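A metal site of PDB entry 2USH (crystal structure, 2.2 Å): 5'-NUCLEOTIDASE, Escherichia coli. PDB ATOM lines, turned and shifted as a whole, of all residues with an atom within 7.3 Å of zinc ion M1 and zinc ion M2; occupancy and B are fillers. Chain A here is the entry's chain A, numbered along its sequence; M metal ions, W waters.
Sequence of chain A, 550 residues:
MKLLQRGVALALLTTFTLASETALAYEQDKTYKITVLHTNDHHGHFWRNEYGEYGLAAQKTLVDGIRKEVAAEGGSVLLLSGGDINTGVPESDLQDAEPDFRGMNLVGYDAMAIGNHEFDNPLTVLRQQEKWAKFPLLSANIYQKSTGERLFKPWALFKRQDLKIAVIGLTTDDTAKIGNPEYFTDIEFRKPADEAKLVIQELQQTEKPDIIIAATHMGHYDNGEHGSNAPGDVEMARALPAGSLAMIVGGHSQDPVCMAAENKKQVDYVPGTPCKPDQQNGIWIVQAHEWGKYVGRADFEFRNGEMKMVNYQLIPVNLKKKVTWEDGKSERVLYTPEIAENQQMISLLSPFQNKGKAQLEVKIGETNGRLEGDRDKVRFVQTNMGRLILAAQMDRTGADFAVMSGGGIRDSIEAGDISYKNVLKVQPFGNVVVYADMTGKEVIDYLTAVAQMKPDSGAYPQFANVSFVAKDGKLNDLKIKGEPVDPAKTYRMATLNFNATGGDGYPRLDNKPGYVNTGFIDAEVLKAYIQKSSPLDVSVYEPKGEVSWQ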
ATOM      1  N   ASN A  40     -26.773   7.578  22.603  1.00  0.00           N
ATOM      2  CA  ASN A  40     -26.954   8.590  23.642  1.00  0.00           C
ATOM      3  C   ASN A  40     -25.858   8.502  24.677  1.00  0.00           C
ATOM      4  O   ASN A  40     -25.183   7.491  24.771  1.00  0.00           O
ATOM      5  CB  ASN A  40     -28.295   8.405  24.364  1.00  0.00           C
ATOM      6  CG  ASN A  40     -28.450   7.016  24.907  1.00  0.00           C
ATOM      7  OD1 ASN A  40     -28.736   6.065  24.155  1.00  0.00           O
ATOM      8  ND2 ASN A  40     -28.241   6.870  26.212  1.00  0.00           N
ATOM      9  N   ASP A  41     -25.680   9.576  25.438  1.00  0.00           N
ATOM     10  CA  ASP A  41     -24.704   9.594  26.521  1.00  0.00           C
ATOM     11  C   ASP A  41     -23.322   9.088  26.140  1.00  0.00           C
ATOM     12  O   ASP A  41     -22.748   8.214  26.797  1.00  0.00           O
ATOM     13  CB  ASP A  41     -25.301   8.798  27.654  1.00  0.00           C
ATOM     14  CG  ASP A  41     -26.615   9.391  28.083  1.00  0.00           C
ATOM     15  OD1 ASP A  41     -27.677   9.035  27.517  1.00  0.00           O
ATOM     16  OD2 ASP A  41     -26.553  10.270  28.960  1.00  0.00           O
ATOM     17  N   HIS A  42     -22.835   9.682  25.056  1.00  0.00           N
ATOM     18  CA  HIS A  42     -21.534   9.460  24.449  1.00  0.00           C
ATOM     19  C   HIS A  42     -20.437   9.764  25.468  1.00  0.00           C
ATOM     20  O   HIS A  42     -19.468   9.026  25.588  1.00  0.00           O
ATOM     21  CB  HIS A  42     -21.402  10.374  23.220  1.00  0.00           C
ATOM     22  CG  HIS A  42     -20.061  10.285  22.553  1.00  0.00           C
ATOM     23  ND1 HIS A  42     -19.638   9.147  21.916  1.00  0.00           N
ATOM     24  CD2 HIS A  42     -19.038  11.165  22.512  1.00  0.00           C
ATOM     25  CE1 HIS A  42     -18.390   9.320  21.507  1.00  0.00           C
ATOM     26  NE2 HIS A  42     -18.001  10.534  21.863  1.00  0.00           N
ATOM     27  N   HIS A  43     -20.606  10.872  26.183  1.00  0.00           N
ATOM     28  CA  HIS A  43     -19.671  11.275  27.221  1.00  0.00           C
ATOM     29  C   HIS A  43     -18.144  11.231  27.008  1.00  0.00           C
ATOM     30  O   HIS A  43     -17.424  10.695  27.827  1.00  0.00           O
ATOM     31  CB  HIS A  43     -20.025  10.552  28.540  1.00  0.00           C
ATOM     32  CG  HIS A  43     -21.307  11.028  29.164  1.00  0.00           C
ATOM     33  ND1 HIS A  43     -21.545  12.357  29.442  1.00  0.00           N
ATOM     34  CD2 HIS A  43     -22.393  10.358  29.605  1.00  0.00           C
ATOM     35  CE1 HIS A  43     -22.713  12.486  30.027  1.00  0.00           C
ATOM     36  NE2 HIS A  43     -23.262  11.287  30.132  1.00  0.00           N
ATOM     37  N   GLY A  82     -29.394  11.026  21.681  1.00  0.00           N
ATOM     38  CA  GLY A  82     -30.139  11.432  22.865  1.00  0.00           C
ATOM     39  C   GLY A  82     -29.376  12.407  23.774  1.00  0.00           C
ATOM     40  O   GLY A  82     -29.792  12.629  24.923  1.00  0.00           O
ATOM     41  N   GLY A  83     -28.256  12.972  23.312  1.00  0.00           N
ATOM     42  CA  GLY A  83     -27.543  13.936  24.138  1.00  0.00           C
ATOM     43  C   GLY A  83     -26.434  13.440  25.057  1.00  0.00           C
ATOM     44  O   GLY A  83     -26.171  12.238  25.119  1.00  0.00           O
ATOM     45  N   ASP A  84     -25.866  14.356  25.844  1.00  0.00           N
ATOM     46  CA  ASP A  84     -24.706  14.079  26.719  1.00  0.00           C
ATOM     47  C   ASP A  84     -23.469  13.599  25.954  1.00  0.00           C
ATOM     48  O   ASP A  84     -23.007  12.476  26.106  1.00  0.00           O
ATOM     49  CB  ASP A  84     -25.034  13.125  27.865  1.00  0.00           C
ATOM     50  CG  ASP A  84     -25.673  13.829  29.042  1.00  0.00           C
ATOM     51  OD1 ASP A  84     -25.812  15.062  28.986  1.00  0.00           O
ATOM     52  OD2 ASP A  84     -26.005  13.173  30.044  1.00  0.00           O
ATOM     53  N   ILE A  85     -22.950  14.489  25.118  1.00  0.00           N
ATOM     54  CA  ILE A  85     -21.776  14.229  24.320  1.00  0.00           C
ATOM     55  C   ILE A  85     -20.610  14.649  25.211  1.00  0.00           C
ATOM     56  O   ILE A  85     -19.538  14.046  25.188  1.00  0.00           O
ATOM     57  CB  ILE A  85     -21.792  15.122  23.040  1.00  0.00           C
ATOM     58  CG1 ILE A  85     -23.131  14.918  22.331  1.00  0.00           C
ATOM     59  CG2 ILE A  85     -20.592  14.820  22.146  1.00  0.00           C
ATOM     60  CD1 ILE A  85     -23.465  13.486  22.015  1.00  0.00           C
ATOM     61  N   ASN A  86     -20.842  15.703  25.996  1.00  0.00           N
ATOM     62  CA  ASN A  86     -19.887  16.276  26.940  1.00  0.00           C
ATOM     63  C   ASN A  86     -19.686  15.497  28.223  1.00  0.00           C
ATOM     64  O   ASN A  86     -20.602  14.844  28.725  1.00  0.00           O
ATOM     65  CB  ASN A  86     -20.300  17.709  27.373  1.00  0.00           C
ATOM     66  CG  ASN A  86     -20.076  18.769  26.291  1.00  0.00           C
ATOM     67  OD1 ASN A  86     -18.993  19.335  26.201  1.00  0.00           O
ATOM     68  ND2 ASN A  86     -21.096  19.080  25.500  1.00  0.00           N
ATOM     69  N   THR A  87     -18.466  15.612  28.750  1.00  0.00           N
ATOM     70  CA  THR A  87     -18.066  15.070  30.056  1.00  0.00           C
ATOM     71  C   THR A  87     -17.936  13.575  30.216  1.00  0.00           C
ATOM     72  O   THR A  87     -18.904  12.861  30.098  1.00  0.00           O
ATOM     73  CB  THR A  87     -19.037  15.565  31.113  1.00  0.00           C
ATOM     74  OG1 THR A  87     -19.110  17.006  31.034  1.00  0.00           O
ATOM     75  CG2 THR A  87     -18.587  15.151  32.511  1.00  0.00           C
ATOM     76  N   GLY A 115     -28.412  17.416  26.199  1.00  0.00           N
ATOM     77  CA  GLY A 115     -28.416  16.749  27.492  1.00  0.00           C
ATOM     78  C   GLY A 115     -28.053  17.641  28.671  1.00  0.00           C
ATOM     79  O   GLY A 115     -27.641  18.784  28.508  1.00  0.00           O
ATOM     80  N   ASN A 116     -28.206  17.130  29.887  1.00  0.00           N
ATOM     81  CA  ASN A 116     -27.882  17.935  31.033  1.00  0.00           C
ATOM     82  C   ASN A 116     -26.383  18.266  31.084  1.00  0.00           C
ATOM     83  O   ASN A 116     -26.002  19.335  31.537  1.00  0.00           O
ATOM     84  CB  ASN A 116     -28.376  17.247  32.324  1.00  0.00           C
ATOM     85  CG  ASN A 116     -27.742  15.889  32.543  1.00  0.00           C
ATOM     86  OD1 ASN A 116     -27.763  15.030  31.674  1.00  0.00           O
ATOM     87  ND2 ASN A 116     -27.185  15.681  33.735  1.00  0.00           N
ATOM     88  N   HIS A 117     -25.531  17.367  30.604  1.00  0.00           N
ATOM     89  CA  HIS A 117     -24.091  17.651  30.620  1.00  0.00           C
ATOM     90  C   HIS A 117     -23.554  18.591  29.527  1.00  0.00           C
ATOM     91  O   HIS A 117     -22.334  18.801  29.443  1.00  0.00           O
ATOM     92  CB  HIS A 117     -23.240  16.361  30.661  1.00  0.00           C
ATOM     93  CG  HIS A 117     -23.296  15.657  31.984  1.00  0.00           C
ATOM     94  ND1 HIS A 117     -22.523  16.045  33.061  1.00  0.00           N
ATOM     95  CD2 HIS A 117     -24.092  14.654  32.441  1.00  0.00           C
ATOM     96  CE1 HIS A 117     -22.854  15.339  34.124  1.00  0.00           C
ATOM     97  NE2 HIS A 117     -23.795  14.489  33.774  1.00  0.00           N
ATOM     98  N   THR A 172     -34.137  17.188  30.176  1.00  0.00           N
ATOM     99  CA  THR A 172     -34.560  17.036  31.574  1.00  0.00           C
ATOM    100  C   THR A 172     -34.469  18.352  32.330  1.00  0.00           C
ATOM    101  O   THR A 172     -33.486  19.093  32.241  1.00  0.00           O
ATOM    102  CB  THR A 172     -33.718  15.962  32.348  1.00  0.00           C
ATOM    103  OG1 THR A 172     -34.214  15.874  33.691  1.00  0.00           O
ATOM    104  CG2 THR A 172     -32.244  16.323  32.377  1.00  0.00           C
ATOM    105  N   THR A 175     -31.647  19.376  35.043  1.00  0.00           N
ATOM    106  CA  THR A 175     -30.369  19.942  34.682  1.00  0.00           C
ATOM    107  C   THR A 175     -29.930  21.010  35.643  1.00  0.00           C
ATOM    108  O   THR A 175     -28.761  21.093  35.926  1.00  0.00           O
ATOM    109  CB  THR A 175     -30.406  20.472  33.248  1.00  0.00           C
ATOM    110  OG1 THR A 175     -30.616  19.352  32.374  1.00  0.00           O
ATOM    111  CG2 THR A 175     -29.083  21.198  32.885  1.00  0.00           C
ATOM    112  N   HIS A 217     -33.702  13.841  26.441  1.00  0.00           N
ATOM    113  CA  HIS A 217     -32.668  13.488  27.400  1.00  0.00           C
ATOM    114  C   HIS A 217     -33.341  13.573  28.780  1.00  0.00           C
ATOM    115  O   HIS A 217     -33.093  14.488  29.562  1.00  0.00           O
ATOM    116  CB  HIS A 217     -31.504  14.438  27.278  1.00  0.00           C
ATOM    117  CG  HIS A 217     -30.323  13.962  28.026  1.00  0.00           C
ATOM    118  ND1 HIS A 217     -29.431  13.075  27.465  1.00  0.00           N
ATOM    119  CD2 HIS A 217     -29.959  14.118  29.316  1.00  0.00           C
ATOM    120  CE1 HIS A 217     -28.572  12.695  28.390  1.00  0.00           C
ATOM    121  NE2 HIS A 217     -28.879  13.301  29.524  1.00  0.00           N
ATOM    122  N   MET A 218     -34.198  12.580  29.059  1.00  0.00           N
ATOM    123  CA  MET A 218     -35.012  12.573  30.281  1.00  0.00           C
ATOM    124  C   MET A 218     -34.907  11.313  31.149  1.00  0.00           C
ATOM    125  O   MET A 218     -35.112  11.388  32.352  1.00  0.00           O
ATOM    126  CB  MET A 218     -36.471  12.856  29.866  1.00  0.00           C
ATOM    127  CG  MET A 218     -36.638  14.229  29.138  1.00  0.00           C
ATOM    128  SD  MET A 218     -38.242  14.486  28.324  1.00  0.00           S
ATOM    129  CE  MET A 218     -39.401  13.735  29.475  1.00  0.00           C
ATOM    130  N   GLY A 251     -32.343   8.965  26.548  1.00  0.00           N
ATOM    131  CA  GLY A 251     -31.017   8.973  27.151  1.00  0.00           C
ATOM    132  C   GLY A 251     -31.073   9.376  28.614  1.00  0.00           C
ATOM    133  O   GLY A 251     -32.127   9.282  29.259  1.00  0.00           O
ATOM    134  N   HIS A 252     -29.932   9.782  29.145  1.00  0.00           N
ATOM    135  CA  HIS A 252     -29.809  10.281  30.501  1.00  0.00           C
ATOM    136  C   HIS A 252     -29.741   9.227  31.585  1.00  0.00           C
ATOM    137  O   HIS A 252     -28.817   9.235  32.397  1.00  0.00           O
ATOM    138  CB  HIS A 252     -30.945  11.268  30.820  1.00  0.00           C
ATOM    139  CG  HIS A 252     -30.782  11.957  32.145  1.00  0.00           C
ATOM    140  ND1 HIS A 252     -29.644  12.647  32.476  1.00  0.00           N
ATOM    141  CD2 HIS A 252     -31.612  12.063  33.207  1.00  0.00           C
ATOM    142  CE1 HIS A 252     -29.773  13.147  33.689  1.00  0.00           C
ATOM    143  NE2 HIS A 252     -30.949  12.809  34.153  1.00  0.00           N
ATOM    144  N   SER A 253     -30.737   8.356  31.638  1.00  0.00           N
ATOM    145  CA  SER A 253     -30.717   7.279  32.614  1.00  0.00           C
ATOM    146  C   SER A 253     -29.596   6.294  32.231  1.00  0.00           C
ATOM    147  O   SER A 253     -29.091   5.597  33.077  1.00  0.00           O
ATOM    148  CB  SER A 253     -32.081   6.563  32.699  1.00  0.00           C
ATOM    149  OG  SER A 253     -32.522   6.002  31.466  1.00  0.00           O
ATOM    150  N   GLN A 254     -29.225   6.247  30.946  1.00  0.00           N
ATOM    151  CA  GLN A 254     -28.172   5.383  30.435  1.00  0.00           C
ATOM    152  C   GLN A 254     -28.355   3.891  30.596  1.00  0.00           C
ATOM    153  O   GLN A 254     -27.478   3.192  31.092  1.00  0.00           O
ATOM    154  CB  GLN A 254     -26.819   5.814  31.009  1.00  0.00           C
ATOM    155  CG  GLN A 254     -26.497   7.246  30.609  1.00  0.00           C
ATOM    156  CD  GLN A 254     -25.189   7.751  31.187  1.00  0.00           C
ATOM    157  OE1 GLN A 254     -25.040   8.942  31.465  1.00  0.00           O
ATOM    158  NE2 GLN A 254     -24.227   6.844  31.353  1.00  0.00           N
ATOM    159  N   HIS A 289     -28.120   2.755  26.060  1.00  0.00           N
ATOM    160  CA  HIS A 289     -27.165   2.652  27.127  1.00  0.00           C
ATOM    161  C   HIS A 289     -26.199   3.846  27.228  1.00  0.00           C
ATOM    162  O   HIS A 289     -26.603   4.921  27.676  1.00  0.00           O
ATOM    163  CB  HIS A 289     -26.407   1.341  26.933  1.00  0.00           C
ATOM    164  CG  HIS A 289     -25.519   0.983  28.067  1.00  0.00           C
ATOM    165  ND1 HIS A 289     -25.805   1.326  29.369  1.00  0.00           N
ATOM    166  CD2 HIS A 289     -24.368   0.265  28.108  1.00  0.00           C
ATOM    167  CE1 HIS A 289     -24.870   0.831  30.170  1.00  0.00           C
ATOM    168  NE2 HIS A 289     -23.995   0.179  29.423  1.00  0.00           N
ATOM    169  N   GLU A 290     -24.942   3.711  26.820  1.00  0.00           N
ATOM    170  CA  GLU A 290     -24.053   4.842  26.977  1.00  0.00           C
ATOM    171  C   GLU A 290     -22.734   4.575  26.267  1.00  0.00           C
ATOM    172  O   GLU A 290     -22.459   3.453  25.873  1.00  0.00           O
ATOM    173  CB  GLU A 290     -23.718   5.023  28.472  1.00  0.00           C
ATOM    174  CG  GLU A 290     -22.838   3.845  28.939  1.00  0.00           C
ATOM    175  CD  GLU A 290     -22.692   3.710  30.430  1.00  0.00           C
ATOM    176  OE1 GLU A 290     -23.401   4.408  31.179  1.00  0.00           O
ATOM    177  OE2 GLU A 290     -21.870   2.878  30.844  1.00  0.00           O
ATOM    178  N   TRP A 291     -21.936   5.653  26.142  1.00  0.00           N
ATOM    179  CA  TRP A 291     -20.573   5.636  25.599  1.00  0.00           C
ATOM    180  C   TRP A 291     -20.263   5.087  24.205  1.00  0.00           C
ATOM    181  O   TRP A 291     -19.112   4.733  23.932  1.00  0.00           O
ATOM    182  CB  TRP A 291     -19.654   4.891  26.584  1.00  0.00           C
ATOM    183  CG  TRP A 291     -19.658   5.444  27.996  1.00  0.00           C
ATOM    184  CD1 TRP A 291     -20.302   6.560  28.455  1.00  0.00           C
ATOM    185  CD2 TRP A 291     -19.005   4.850  29.143  1.00  0.00           C
ATOM    186  NE1 TRP A 291     -20.093   6.702  29.807  1.00  0.00           N
ATOM    187  CE2 TRP A 291     -19.302   5.668  30.251  1.00  0.00           C
ATOM    188  CE3 TRP A 291     -18.198   3.711  29.331  1.00  0.00           C
ATOM    189  CZ2 TRP A 291     -18.820   5.379  31.554  1.00  0.00           C
ATOM    190  CZ3 TRP A 291     -17.716   3.426  30.617  1.00  0.00           C
ATOM    191  CH2 TRP A 291     -18.031   4.269  31.713  1.00  0.00           C
ATOM    192  N   THR A 518     -24.340  11.585  39.428  1.00  0.00           N
ATOM    193  CA  THR A 518     -24.063  12.896  38.801  1.00  0.00           C
ATOM    194  C   THR A 518     -23.454  12.815  37.424  1.00  0.00           C
ATOM    195  O   THR A 518     -23.491  13.776  36.680  1.00  0.00           O
ATOM    196  CB  THR A 518     -23.101  13.744  39.620  1.00  0.00           C
ATOM    197  OG1 THR A 518     -21.821  13.079  39.666  1.00  0.00           O
ATOM    198  CG2 THR A 518     -23.630  13.932  41.038  1.00  0.00           C
ATOM    199  N   GLY A 519     -22.877  11.678  37.081  1.00  0.00           N
ATOM    200  CA  GLY A 519     -22.241  11.618  35.788  1.00  0.00           C
ATOM    201  C   GLY A 519     -20.862  12.283  35.829  1.00  0.00           C
ATOM    202  O   GLY A 519     -20.216  12.355  34.796  1.00  0.00           O
HETATM  203 ZN    ZN M   1     -25.379  10.997  30.559  1.00  0.00          ZN
HETATM  204 ZN    ZN M   2     -27.869  13.079  31.301  1.00  0.00          ZN
HETATM  205  O   HOH W   1     -26.633  11.528  32.085  1.00  0.00           O
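The backbone carbonyl oxygen (O) of His 217 sits at hydrogen-bond distance from the backbone NH (N) of Thr 172, 3.0 Å away.
OD1 of Asp 41 sits at hydrogen-bond distance from N of His 252 (2.9 Å).
The backbone NH (N) of Asp 41 lies within hydrogen-bond range of the backbone carbonyl oxygen (O) of Gly 83, at 2.7 Å.
The side-chain carboxylate (OD1) of Asp 41 is in hydrogen-bond range of the side-chain amide nitrogen (ND2) of Asn 40 (2.6 Å).
The backbone carbonyl oxygen of Asn 86 lies within hydrogen-bond range of a ring nitrogen (ND1) of His 43, at 2.8 Å.
ND1 of His 43 is in hydrogen-bond range of O of Thr 87, 2.8 Å away.
O of Asp 84 is in hydrogen-bond range of N of His 42 (3.0 Å).
The side-chain amide nitrogen of Gln 254 sits at hydrogen-bond distance from the side-chain carboxylate of Glu 290 (2.6 Å).
Water W1 is bound to zinc ion M1 (2.0 Å).
The side-chain carboxylate (OD2) of Asp 41 is bound to zinc ion M1.
A ring nitrogen (NE2) of His 43 is bound to zinc ion M1.
OE1 of Gln 254 is bound to zinc ion M1.
OD2 of Asp 84 is bound to zinc ion M1.
Zinc ion M1 has five donor atoms within binding distance.
Of the 26 residues printed, 5 come within 4 Å of zinc ion M2.
Zinc ion M2 is bound by OD1 of Asn 116.
NE2 of His 217 is bound to zinc ion M2 (2.1 Å).
Water W1 binds zinc ion M2.
ND1 of His 252 is bound to zinc ion M2.
OD2 of Asp 84 is bound to zinc ion M2 (2.3 Å).
Four residues have an atom within 4 Å of zinc ion M1: Asp 41, His 43, Asp 84 and Gln 254.
The nearest printed residue that does not touch zinc ion M1 is His 217 (4.2 Å).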
